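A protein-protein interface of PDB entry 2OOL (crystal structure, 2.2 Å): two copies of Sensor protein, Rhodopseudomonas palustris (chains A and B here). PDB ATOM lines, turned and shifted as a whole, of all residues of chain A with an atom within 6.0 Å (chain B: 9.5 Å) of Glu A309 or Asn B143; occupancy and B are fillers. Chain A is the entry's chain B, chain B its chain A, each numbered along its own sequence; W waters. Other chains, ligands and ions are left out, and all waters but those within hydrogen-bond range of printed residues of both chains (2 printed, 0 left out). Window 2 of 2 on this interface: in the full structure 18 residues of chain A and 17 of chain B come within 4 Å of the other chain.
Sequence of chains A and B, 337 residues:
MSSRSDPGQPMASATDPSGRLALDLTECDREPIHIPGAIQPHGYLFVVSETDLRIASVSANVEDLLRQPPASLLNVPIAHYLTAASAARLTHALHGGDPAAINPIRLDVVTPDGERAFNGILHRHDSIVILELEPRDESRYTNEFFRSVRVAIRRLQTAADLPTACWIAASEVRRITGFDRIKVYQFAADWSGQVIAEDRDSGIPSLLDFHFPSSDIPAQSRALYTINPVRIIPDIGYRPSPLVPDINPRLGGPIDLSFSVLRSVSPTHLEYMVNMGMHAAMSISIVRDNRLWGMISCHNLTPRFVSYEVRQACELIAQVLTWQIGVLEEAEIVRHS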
ATOM      1  N   PRO A 104     -19.680 -26.195   0.419  1.00  0.00           N
ATOM      2  CA  PRO A 104     -19.899 -27.629   0.241  1.00  0.00           C
ATOM      3  C   PRO A 104     -21.069 -27.860  -0.683  1.00  0.00           C
ATOM      4  O   PRO A 104     -21.905 -26.994  -0.811  1.00  0.00           O
ATOM      5  CB  PRO A 104     -20.239 -28.110   1.651  1.00  0.00           C
ATOM      6  CG  PRO A 104     -21.018 -26.920   2.249  1.00  0.00           C
ATOM      7  CD  PRO A 104     -20.446 -25.674   1.571  1.00  0.00           C
ATOM      8  N   ASN A 119     -22.063 -33.665   3.120  1.00  0.00           N
ATOM      9  CA  ASN A 119     -21.327 -32.496   2.603  1.00  0.00           C
ATOM     10  C   ASN A 119     -20.178 -32.929   1.694  1.00  0.00           C
ATOM     11  O   ASN A 119     -19.143 -33.478   2.153  1.00  0.00           O
ATOM     12  CB  ASN A 119     -20.765 -31.624   3.743  1.00  0.00           C
ATOM     13  CG  ASN A 119     -21.726 -30.525   4.199  1.00  0.00           C
ATOM     14  OD1 ASN A 119     -21.494 -29.891   5.243  1.00  0.00           O
ATOM     15  ND2 ASN A 119     -22.788 -30.278   3.417  1.00  0.00           N
ATOM     16  N   PRO A 135     -19.979 -35.599   7.224  1.00  0.00           N
ATOM     17  CA  PRO A 135     -21.306 -35.358   7.801  1.00  0.00           C
ATOM     18  C   PRO A 135     -21.710 -33.898   7.624  1.00  0.00           C
ATOM     19  O   PRO A 135     -20.878 -33.008   7.849  1.00  0.00           O
ATOM     20  CB  PRO A 135     -21.113 -35.677   9.293  1.00  0.00           C
ATOM     21  CG  PRO A 135     -19.906 -36.531   9.349  1.00  0.00           C
ATOM     22  CD  PRO A 135     -19.034 -36.109   8.222  1.00  0.00           C
ATOM     23  N   ARG A 136     -22.956 -33.687   7.191  1.00  0.00           N
ATOM     24  CA  ARG A 136     -23.580 -32.358   7.052  1.00  0.00           C
ATOM     25  C   ARG A 136     -23.803 -31.669   8.388  1.00  0.00           C
ATOM     26  O   ARG A 136     -23.778 -32.325   9.436  1.00  0.00           O
ATOM     27  CB  ARG A 136     -24.948 -32.472   6.382  1.00  0.00           C
ATOM     28  CG  ARG A 136     -24.910 -32.788   4.918  1.00  0.00           C
ATOM     29  CD  ARG A 136     -26.228 -32.438   4.240  1.00  0.00           C
ATOM     30  NE  ARG A 136     -26.355 -31.007   3.962  1.00  0.00           N
ATOM     31  CZ  ARG A 136     -27.513 -30.388   3.725  1.00  0.00           C
ATOM     32  NH1 ARG A 136     -28.663 -31.080   3.747  1.00  0.00           N
ATOM     33  NH2 ARG A 136     -27.541 -29.068   3.477  1.00  0.00           N
ATOM     34  N   ASP A 137     -24.078 -30.356   8.318  1.00  0.00           N
ATOM     35  CA  ASP A 137     -24.323 -29.494   9.498  1.00  0.00           C
ATOM     36  C   ASP A 137     -25.435 -30.002  10.436  1.00  0.00           C
ATOM     37  O   ASP A 137     -26.414 -30.610   9.985  1.00  0.00           O
ATOM     38  CB  ASP A 137     -24.658 -28.050   9.068  1.00  0.00           C
ATOM     39  CG  ASP A 137     -24.473 -27.027  10.207  1.00  0.00           C
ATOM     40  OD1 ASP A 137     -23.429 -27.086  10.908  1.00  0.00           O
ATOM     41  OD2 ASP A 137     -25.377 -26.156  10.404  1.00  0.00           O
ATOM     42  N   PHE A 145     -26.858 -19.639  15.553  1.00  0.00           N
ATOM     43  CA  PHE A 145     -25.582 -19.741  14.870  1.00  0.00           C
ATOM     44  C   PHE A 145     -25.249 -18.517  13.997  1.00  0.00           C
ATOM     45  O   PHE A 145     -24.195 -17.930  14.169  1.00  0.00           O
ATOM     46  CB  PHE A 145     -25.554 -21.039  14.041  1.00  0.00           C
ATOM     47  CG  PHE A 145     -24.382 -21.147  13.115  1.00  0.00           C
ATOM     48  CD1 PHE A 145     -23.141 -21.542  13.589  1.00  0.00           C
ATOM     49  CD2 PHE A 145     -24.518 -20.850  11.764  1.00  0.00           C
ATOM     50  CE1 PHE A 145     -22.046 -21.630  12.732  1.00  0.00           C
ATOM     51  CE2 PHE A 145     -23.431 -20.968  10.887  1.00  0.00           C
ATOM     52  CZ  PHE A 145     -22.190 -21.339  11.370  1.00  0.00           C
ATOM     53  N   PHE A 146     -26.119 -18.160  13.052  1.00  0.00           N
ATOM     54  CA  PHE A 146     -25.869 -17.017  12.165  1.00  0.00           C
ATOM     55  C   PHE A 146     -25.771 -15.698  12.948  1.00  0.00           C
ATOM     56  O   PHE A 146     -24.922 -14.857  12.652  1.00  0.00           O
ATOM     57  CB  PHE A 146     -26.970 -16.855  11.111  1.00  0.00           C
ATOM     58  CG  PHE A 146     -27.218 -18.084  10.266  1.00  0.00           C
ATOM     59  CD1 PHE A 146     -26.191 -18.687   9.572  1.00  0.00           C
ATOM     60  CD2 PHE A 146     -28.506 -18.600  10.150  1.00  0.00           C
ATOM     61  CE1 PHE A 146     -26.425 -19.825   8.796  1.00  0.00           C
ATOM     62  CE2 PHE A 146     -28.767 -19.713   9.388  1.00  0.00           C
ATOM     63  CZ  PHE A 146     -27.725 -20.337   8.698  1.00  0.00           C
ATOM     64  N   SER A 307     -18.944 -29.093  11.626  1.00  0.00           N
ATOM     65  CA  SER A 307     -19.254 -29.164  10.208  1.00  0.00           C
ATOM     66  C   SER A 307     -18.468 -28.155   9.370  1.00  0.00           C
ATOM     67  O   SER A 307     -18.012 -27.119   9.866  1.00  0.00           O
ATOM     68  CB  SER A 307     -20.757 -28.938   9.976  1.00  0.00           C
ATOM     69  OG  SER A 307     -21.088 -27.550  10.106  1.00  0.00           O
ATOM     70  N   TYR A 308     -18.357 -28.461   8.081  1.00  0.00           N
ATOM     71  CA  TYR A 308     -17.684 -27.591   7.130  1.00  0.00           C
ATOM     72  C   TYR A 308     -18.121 -26.146   7.298  1.00  0.00           C
ATOM     73  O   TYR A 308     -17.300 -25.247   7.250  1.00  0.00           O
ATOM     74  CB  TYR A 308     -17.959 -28.066   5.693  1.00  0.00           C
ATOM     75  CG  TYR A 308     -17.109 -27.383   4.643  1.00  0.00           C
ATOM     76  CD1 TYR A 308     -15.800 -27.786   4.396  1.00  0.00           C
ATOM     77  CD2 TYR A 308     -17.618 -26.339   3.900  1.00  0.00           C
ATOM     78  CE1 TYR A 308     -15.021 -27.141   3.423  1.00  0.00           C
ATOM     79  CE2 TYR A 308     -16.859 -25.706   2.940  1.00  0.00           C
ATOM     80  CZ  TYR A 308     -15.578 -26.097   2.714  1.00  0.00           C
ATOM     81  OH  TYR A 308     -14.868 -25.443   1.751  1.00  0.00           O
ATOM     82  N   GLU A 309     -19.425 -25.958   7.510  1.00  0.00           N
ATOM     83  CA  GLU A 309     -20.054 -24.634   7.647  1.00  0.00           C
ATOM     84  C   GLU A 309     -19.597 -23.881   8.866  1.00  0.00           C
ATOM     85  O   GLU A 309     -19.405 -22.676   8.760  1.00  0.00           O
ATOM     86  CB  GLU A 309     -21.572 -24.742   7.687  1.00  0.00           C
ATOM     87  CG  GLU A 309     -22.215 -25.069   6.338  1.00  0.00           C
ATOM     88  CD  GLU A 309     -22.555 -26.560   6.164  1.00  0.00           C
ATOM     89  OE1 GLU A 309     -22.044 -27.421   6.952  1.00  0.00           O
ATOM     90  OE2 GLU A 309     -23.356 -26.848   5.235  1.00  0.00           O
ATOM     91  N   VAL A 310     -19.414 -24.560  10.017  1.00  0.00           N
ATOM     92  CA  VAL A 310     -18.902 -23.839  11.195  1.00  0.00           C
ATOM     93  C   VAL A 310     -17.436 -23.501  10.984  1.00  0.00           C
ATOM     94  O   VAL A 310     -17.031 -22.366  11.239  1.00  0.00           O
ATOM     95  CB  VAL A 310     -19.192 -24.481  12.651  1.00  0.00           C
ATOM     96  CG1 VAL A 310     -20.548 -25.176  12.719  1.00  0.00           C
ATOM     97  CG2 VAL A 310     -18.102 -25.390  13.089  1.00  0.00           C
ATOM     98  N   ARG A 311     -16.648 -24.461  10.482  1.00  0.00           N
ATOM     99  CA  ARG A 311     -15.228 -24.199  10.181  1.00  0.00           C
ATOM    100  C   ARG A 311     -15.074 -23.009   9.219  1.00  0.00           C
ATOM    101  O   ARG A 311     -14.176 -22.198   9.398  1.00  0.00           O
ATOM    102  CB  ARG A 311     -14.507 -25.443   9.611  1.00  0.00           C
ATOM    103  CG  ARG A 311     -14.655 -26.722  10.438  1.00  0.00           C
ATOM    104  CD  ARG A 311     -13.553 -27.746  10.228  1.00  0.00           C
ATOM    105  NE  ARG A 311     -13.441 -28.294   8.874  1.00  0.00           N
ATOM    106  CZ  ARG A 311     -14.289 -29.154   8.299  1.00  0.00           C
ATOM    107  NH1 ARG A 311     -15.403 -29.559   8.917  1.00  0.00           N
ATOM    108  NH2 ARG A 311     -14.036 -29.595   7.066  1.00  0.00           N
ATOM    109  N   GLN A 312     -15.944 -22.916   8.217  1.00  0.00           N
ATOM    110  CA  GLN A 312     -15.966 -21.765   7.317  1.00  0.00           C
ATOM    111  C   GLN A 312     -16.328 -20.456   8.080  1.00  0.00           C
ATOM    112  O   GLN A 312     -15.725 -19.401   7.845  1.00  0.00           O
ATOM    113  CB  GLN A 312     -16.974 -21.968   6.167  1.00  0.00           C
ATOM    114  CG  GLN A 312     -16.549 -22.892   5.040  1.00  0.00           C
ATOM    115  CD  GLN A 312     -15.298 -22.408   4.277  1.00  0.00           C
ATOM    116  OE1 GLN A 312     -14.147 -22.717   4.662  1.00  0.00           O
ATOM    117  NE2 GLN A 312     -15.522 -21.652   3.182  1.00  0.00           N
ATOM    118  N   ALA A 313     -17.325 -20.532   8.970  1.00  0.00           N
ATOM    119  CA  ALA A 313     -17.629 -19.416   9.864  1.00  0.00           C
ATOM    120  C   ALA A 313     -16.385 -18.985  10.660  1.00  0.00           C
ATOM    121  O   ALA A 313     -16.050 -17.803  10.653  1.00  0.00           O
ATOM    122  CB  ALA A 313     -18.760 -19.763  10.780  1.00  0.00           C
ATOM    123  N   CYS A 314     -15.679 -19.932  11.287  1.00  0.00           N
ATOM    124  CA  CYS A 314     -14.471 -19.618  12.052  1.00  0.00           C
ATOM    125  C   CYS A 314     -13.384 -18.992  11.189  1.00  0.00           C
ATOM    126  O   CYS A 314     -12.489 -18.283  11.674  1.00  0.00           O
ATOM    127  CB  CYS A 314     -13.885 -20.894  12.654  1.00  0.00           C
ATOM    128  SG  CYS A 314     -14.816 -21.630  14.038  1.00  0.00           S
ATOM    129  N   ASP B 137     -34.381  -9.749   7.944  1.00  0.00           N
ATOM    130  CA  ASP B 137     -33.559 -10.380   6.953  1.00  0.00           C
ATOM    131  C   ASP B 137     -34.227 -11.660   6.456  1.00  0.00           C
ATOM    132  O   ASP B 137     -34.700 -12.474   7.261  1.00  0.00           O
ATOM    133  CB  ASP B 137     -32.183 -10.700   7.529  1.00  0.00           C
ATOM    134  CG  ASP B 137     -31.231 -11.232   6.475  1.00  0.00           C
ATOM    135  OD1 ASP B 137     -30.645 -10.426   5.712  1.00  0.00           O
ATOM    136  OD2 ASP B 137     -31.078 -12.464   6.416  1.00  0.00           O
ATOM    137  N   SER B 139     -32.857 -14.145   4.048  1.00  0.00           N
ATOM    138  CA  SER B 139     -32.091 -15.049   3.131  1.00  0.00           C
ATOM    139  C   SER B 139     -32.203 -16.550   3.429  1.00  0.00           C
ATOM    140  O   SER B 139     -32.103 -17.017   4.563  1.00  0.00           O
ATOM    141  CB  SER B 139     -30.616 -14.647   2.973  1.00  0.00           C
ATOM    142  OG  SER B 139     -29.969 -15.510   2.024  1.00  0.00           O
ATOM    143  N   ARG B 140     -32.369 -17.321   2.366  1.00  0.00           N
ATOM    144  CA  ARG B 140     -32.271 -18.758   2.489  1.00  0.00           C
ATOM    145  C   ARG B 140     -30.805 -19.201   2.253  1.00  0.00           C
ATOM    146  O   ARG B 140     -30.556 -20.411   2.110  1.00  0.00           O
ATOM    147  CB  ARG B 140     -33.225 -19.464   1.500  1.00  0.00           C
ATOM    148  CG  ARG B 140     -34.618 -18.788   1.278  1.00  0.00           C
ATOM    149  CD  ARG B 140     -35.393 -19.551   0.151  1.00  0.00           C
ATOM    150  NE  ARG B 140     -36.598 -18.868  -0.374  1.00  0.00           N
ATOM    151  CZ  ARG B 140     -37.349 -19.344  -1.376  1.00  0.00           C
ATOM    152  NH1 ARG B 140     -37.021 -20.492  -1.963  1.00  0.00           N
ATOM    153  NH2 ARG B 140     -38.425 -18.678  -1.802  1.00  0.00           N
ATOM    154  N   TYR B 141     -29.853 -18.249   2.214  1.00  0.00           N
ATOM    155  CA  TYR B 141     -28.461 -18.525   1.732  1.00  0.00           C
ATOM    156  C   TYR B 141     -27.353 -17.822   2.541  1.00  0.00           C
ATOM    157  O   TYR B 141     -26.398 -17.264   1.958  1.00  0.00           O
ATOM    158  CB  TYR B 141     -28.357 -18.168   0.218  1.00  0.00           C
ATOM    159  CG  TYR B 141     -29.404 -18.911  -0.592  1.00  0.00           C
ATOM    160  CD1 TYR B 141     -29.460 -20.306  -0.545  1.00  0.00           C
ATOM    161  CD2 TYR B 141     -30.380 -18.237  -1.338  1.00  0.00           C
ATOM    162  CE1 TYR B 141     -30.433 -21.026  -1.240  1.00  0.00           C
ATOM    163  CE2 TYR B 141     -31.380 -18.963  -2.051  1.00  0.00           C
ATOM    164  CZ  TYR B 141     -31.392 -20.350  -1.983  1.00  0.00           C
ATOM    165  OH  TYR B 141     -32.340 -21.113  -2.641  1.00  0.00           O
ATOM    166  N   THR B 142     -27.485 -17.880   3.877  1.00  0.00           N
ATOM    167  CA  THR B 142     -26.610 -17.149   4.792  1.00  0.00           C
ATOM    168  C   THR B 142     -25.186 -17.743   4.821  1.00  0.00           C
ATOM    169  O   THR B 142     -24.205 -16.986   4.845  1.00  0.00           O
ATOM    170  CB  THR B 142     -27.208 -17.048   6.254  1.00  0.00           C
ATOM    171  OG1 THR B 142     -28.554 -16.541   6.215  1.00  0.00           O
ATOM    172  CG2 THR B 142     -26.354 -16.135   7.149  1.00  0.00           C
ATOM    173  N   ASN B 143     -25.060 -19.071   4.766  1.00  0.00           N
ATOM    174  CA  ASN B 143     -23.716 -19.704   4.693  1.00  0.00           C
ATOM    175  C   ASN B 143     -22.899 -19.295   3.422  1.00  0.00           C
ATOM    176  O   ASN B 143     -21.709 -18.945   3.519  1.00  0.00           O
ATOM    177  CB  ASN B 143     -23.811 -21.228   4.856  1.00  0.00           C
ATOM    178  CG  ASN B 143     -24.092 -21.649   6.320  1.00  0.00           C
ATOM    179  OD1 ASN B 143     -23.500 -21.119   7.268  1.00  0.00           O
ATOM    180  ND2 ASN B 143     -24.985 -22.618   6.494  1.00  0.00           N
ATOM    181  N   GLU B 144     -23.550 -19.333   2.262  1.00  0.00           N
ATOM    182  CA  GLU B 144     -22.994 -18.766   1.028  1.00  0.00           C
ATOM    183  C   GLU B 144     -22.673 -17.276   1.185  1.00  0.00           C
ATOM    184  O   GLU B 144     -21.651 -16.791   0.704  1.00  0.00           O
ATOM    185  CB  GLU B 144     -23.972 -18.954  -0.136  1.00  0.00           C
ATOM    186  N   PHE B 145     -23.564 -16.553   1.841  1.00  0.00           N
ATOM    187  CA  PHE B 145     -23.352 -15.151   2.114  1.00  0.00           C
ATOM    188  C   PHE B 145     -22.045 -14.925   2.871  1.00  0.00           C
ATOM    189  O   PHE B 145     -21.238 -14.116   2.434  1.00  0.00           O
ATOM    190  CB  PHE B 145     -24.530 -14.644   2.941  1.00  0.00           C
ATOM    191  CG  PHE B 145     -24.437 -13.222   3.339  1.00  0.00           C
ATOM    192  CD1 PHE B 145     -24.739 -12.221   2.438  1.00  0.00           C
ATOM    193  CD2 PHE B 145     -24.141 -12.874   4.649  1.00  0.00           C
ATOM    194  CE1 PHE B 145     -24.700 -10.886   2.825  1.00  0.00           C
ATOM    195  CE2 PHE B 145     -24.121 -11.522   5.054  1.00  0.00           C
ATOM    196  CZ  PHE B 145     -24.392 -10.540   4.130  1.00  0.00           C
ATOM    197  N   PHE B 146     -21.849 -15.642   3.984  1.00  0.00           N
ATOM    198  CA  PHE B 146     -20.624 -15.511   4.773  1.00  0.00           C
ATOM    199  C   PHE B 146     -19.373 -15.854   3.945  1.00  0.00           C
ATOM    200  O   PHE B 146     -18.346 -15.181   4.029  1.00  0.00           O
ATOM    201  CB  PHE B 146     -20.633 -16.428   5.991  1.00  0.00           C
ATOM    202  CG  PHE B 146     -21.608 -16.043   7.075  1.00  0.00           C
ATOM    203  CD1 PHE B 146     -22.170 -14.780   7.163  1.00  0.00           C
ATOM    204  CD2 PHE B 146     -21.942 -16.980   8.040  1.00  0.00           C
ATOM    205  CE1 PHE B 146     -23.068 -14.477   8.189  1.00  0.00           C
ATOM    206  CE2 PHE B 146     -22.816 -16.691   9.041  1.00  0.00           C
ATOM    207  CZ  PHE B 146     -23.384 -15.429   9.131  1.00  0.00           C
ATOM    208  N   ARG B 147     -19.464 -16.917   3.164  1.00  0.00           N
ATOM    209  CA  ARG B 147     -18.356 -17.337   2.309  1.00  0.00           C
ATOM    210  C   ARG B 147     -17.970 -16.246   1.318  1.00  0.00           C
ATOM    211  O   ARG B 147     -16.792 -15.936   1.192  1.00  0.00           O
ATOM    212  CB  ARG B 147     -18.731 -18.642   1.567  1.00  0.00           C
ATOM    213  CG  ARG B 147     -17.759 -19.103   0.522  1.00  0.00           C
ATOM    214  CD  ARG B 147     -18.279 -20.366  -0.105  1.00  0.00           C
ATOM    215  NE  ARG B 147     -19.434 -20.117  -0.967  1.00  0.00           N
ATOM    216  CZ  ARG B 147     -20.418 -20.993  -1.210  1.00  0.00           C
ATOM    217  NH1 ARG B 147     -20.437 -22.196  -0.640  1.00  0.00           N
ATOM    218  NH2 ARG B 147     -21.411 -20.654  -2.026  1.00  0.00           N
ATOM    219  N   SER B 148     -18.965 -15.635   0.662  1.00  0.00           N
ATOM    220  CA  SER B 148     -18.671 -14.568  -0.306  1.00  0.00           C
ATOM    221  C   SER B 148     -18.030 -13.353   0.374  1.00  0.00           C
ATOM    222  O   SER B 148     -17.044 -12.827  -0.124  1.00  0.00           O
ATOM    223  CB  SER B 148     -19.900 -14.153  -1.163  1.00  0.00           C
ATOM    224  OG  SER B 148     -20.881 -13.486  -0.402  1.00  0.00           O
ATOM    225  N   VAL B 149     -18.558 -12.919   1.522  1.00  0.00           N
ATOM    226  CA  VAL B 149     -17.918 -11.813   2.271  1.00  0.00           C
ATOM    227  C   VAL B 149     -16.441 -12.144   2.638  1.00  0.00           C
ATOM    228  O   VAL B 149     -15.535 -11.339   2.433  1.00  0.00           O
ATOM    229  CB  VAL B 149     -18.729 -11.389   3.510  1.00  0.00           C
ATOM    230  CG1 VAL B 149     -17.910 -10.418   4.374  1.00  0.00           C
ATOM    231  CG2 VAL B 149     -20.070 -10.755   3.100  1.00  0.00           C
ATOM    232  N   ARG B 150     -16.196 -13.363   3.100  1.00  0.00           N
ATOM    233  CA  ARG B 150     -14.843 -13.811   3.447  1.00  0.00           C
ATOM    234  C   ARG B 150     -13.851 -13.794   2.248  1.00  0.00           C
ATOM    235  O   ARG B 150     -12.717 -13.294   2.379  1.00  0.00           O
ATOM    236  CB  ARG B 150     -14.901 -15.203   4.104  1.00  0.00           C
ATOM    237  CG  ARG B 150     -13.518 -15.794   4.396  1.00  0.00           C
ATOM    238  CD  ARG B 150     -13.564 -17.243   4.884  1.00  0.00           C
ATOM    239  NE  ARG B 150     -13.860 -18.209   3.819  1.00  0.00           N
ATOM    240  CZ  ARG B 150     -13.000 -18.604   2.886  1.00  0.00           C
ATOM    241  NH1 ARG B 150     -13.394 -19.491   1.977  1.00  0.00           N
ATOM    242  NH2 ARG B 150     -11.760 -18.117   2.834  1.00  0.00           N
ATOM    243  N   VAL B 151     -14.247 -14.344   1.099  1.00  0.00           N
ATOM    244  CA  VAL B 151     -13.311 -14.392  -0.025  1.00  0.00           C
ATOM    245  C   VAL B 151     -13.095 -12.974  -0.585  1.00  0.00           C
ATOM    246  O   VAL B 151     -11.991 -12.619  -0.930  1.00  0.00           O
ATOM    247  CB  VAL B 151     -13.608 -15.523  -1.115  1.00  0.00           C
ATOM    248  CG1 VAL B 151     -14.328 -16.743  -0.521  1.00  0.00           C
ATOM    249  CG2 VAL B 151     -14.303 -14.992  -2.391  1.00  0.00           C
ATOM    250  N   GLU B 172     -18.747  -7.379  -5.098  1.00  0.00           N
ATOM    251  CA  GLU B 172     -19.296  -8.121  -3.947  1.00  0.00           C
ATOM    252  C   GLU B 172     -20.555  -7.465  -3.377  1.00  0.00           C
ATOM    253  O   GLU B 172     -21.513  -8.138  -3.019  1.00  0.00           O
ATOM    254  CB  GLU B 172     -18.261  -8.282  -2.837  1.00  0.00           C
ATOM    255  CG  GLU B 172     -18.854  -8.912  -1.507  1.00  0.00           C
ATOM    256  CD  GLU B 172     -19.086 -10.427  -1.609  1.00  0.00           C
ATOM    257  OE1 GLU B 172     -18.721 -11.030  -2.626  1.00  0.00           O
ATOM    258  OE2 GLU B 172     -19.606 -11.031  -0.650  1.00  0.00           O
HETATM  259  O   HOH W   1     -20.599 -20.647   7.500  1.00  0.00           O
HETATM  260  O   HOH W   2     -16.779 -18.285   5.368  1.00  0.00           O
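Among the printed residues, merely in contact across the chains: Phe A146 with Thr B142 (3.5 Å), Phe A146 with Asn B143 (3.5 Å), Phe A145 with Asn B143 (3.6 Å), Glu A309 with Asn B143 (3.7 Å) and Phe A146 with Phe B146 (3.9 Å).
Water W1 bridges the backbone carbonyl oxygen of Glu A309 (2.7 Å) and the side-chain amide oxygen of Asn B143 (2.9 Å). Water W2 bridges O of Gln A312 (2.9 Å) and NE of Arg B150 (3.3 Å).
Glu A309 touches just one residue of chain B: Asn B143. Asn B143 touches three residues of chain A. No residue of chain B comes within 4 Å of Ser A307. No residue of chain B comes within 4 Å of Val A310. Of the printed residues of chain A, Phe B146 touches Phe A146 (3.9 Å). Printed residues of chain B within 4 Å of Gln A312: Arg B150 (3.3 Å). The nearest printed residue of chain B that does not touch Phe A145 is Phe B146 (4.7 Å).
OD1 of Asn A119 lies close to OE1 of Glu A309 (3.1 Å). The side-chain hydroxyl (OG) of Ser A307 sits at hydrogen-bond distance from the side-chain carboxylate (OE1) of Glu A309 (3.3 Å).
Phe A146 touches its own counterpart, Phe B146. Of the 6 pairs that touch across the chains among the printed residues, 1 has its exchanged pair printed and touching as well.
Of the 15 printed residues of chain B, 4 touch a printed residue of chain A. Of the 15 printed residues of chain A, 4 touch a printed residue of chain B. Printed residues of chain A that touch a printed residue of chain B: Phe A145, Phe A146, Glu A309 and Gln A312. Among the printed residues, 6 pairs touch across the chains. Among the printed residues, no Asp or Glu carboxylate lies within 4 Å of a Lys or Arg side-chain nitrogen of the other chain.
The guanidinium group (NH1) of Arg B150 lies close to the side-chain amide nitrogen (NE2) of Gln A312, at 3.3 Å.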
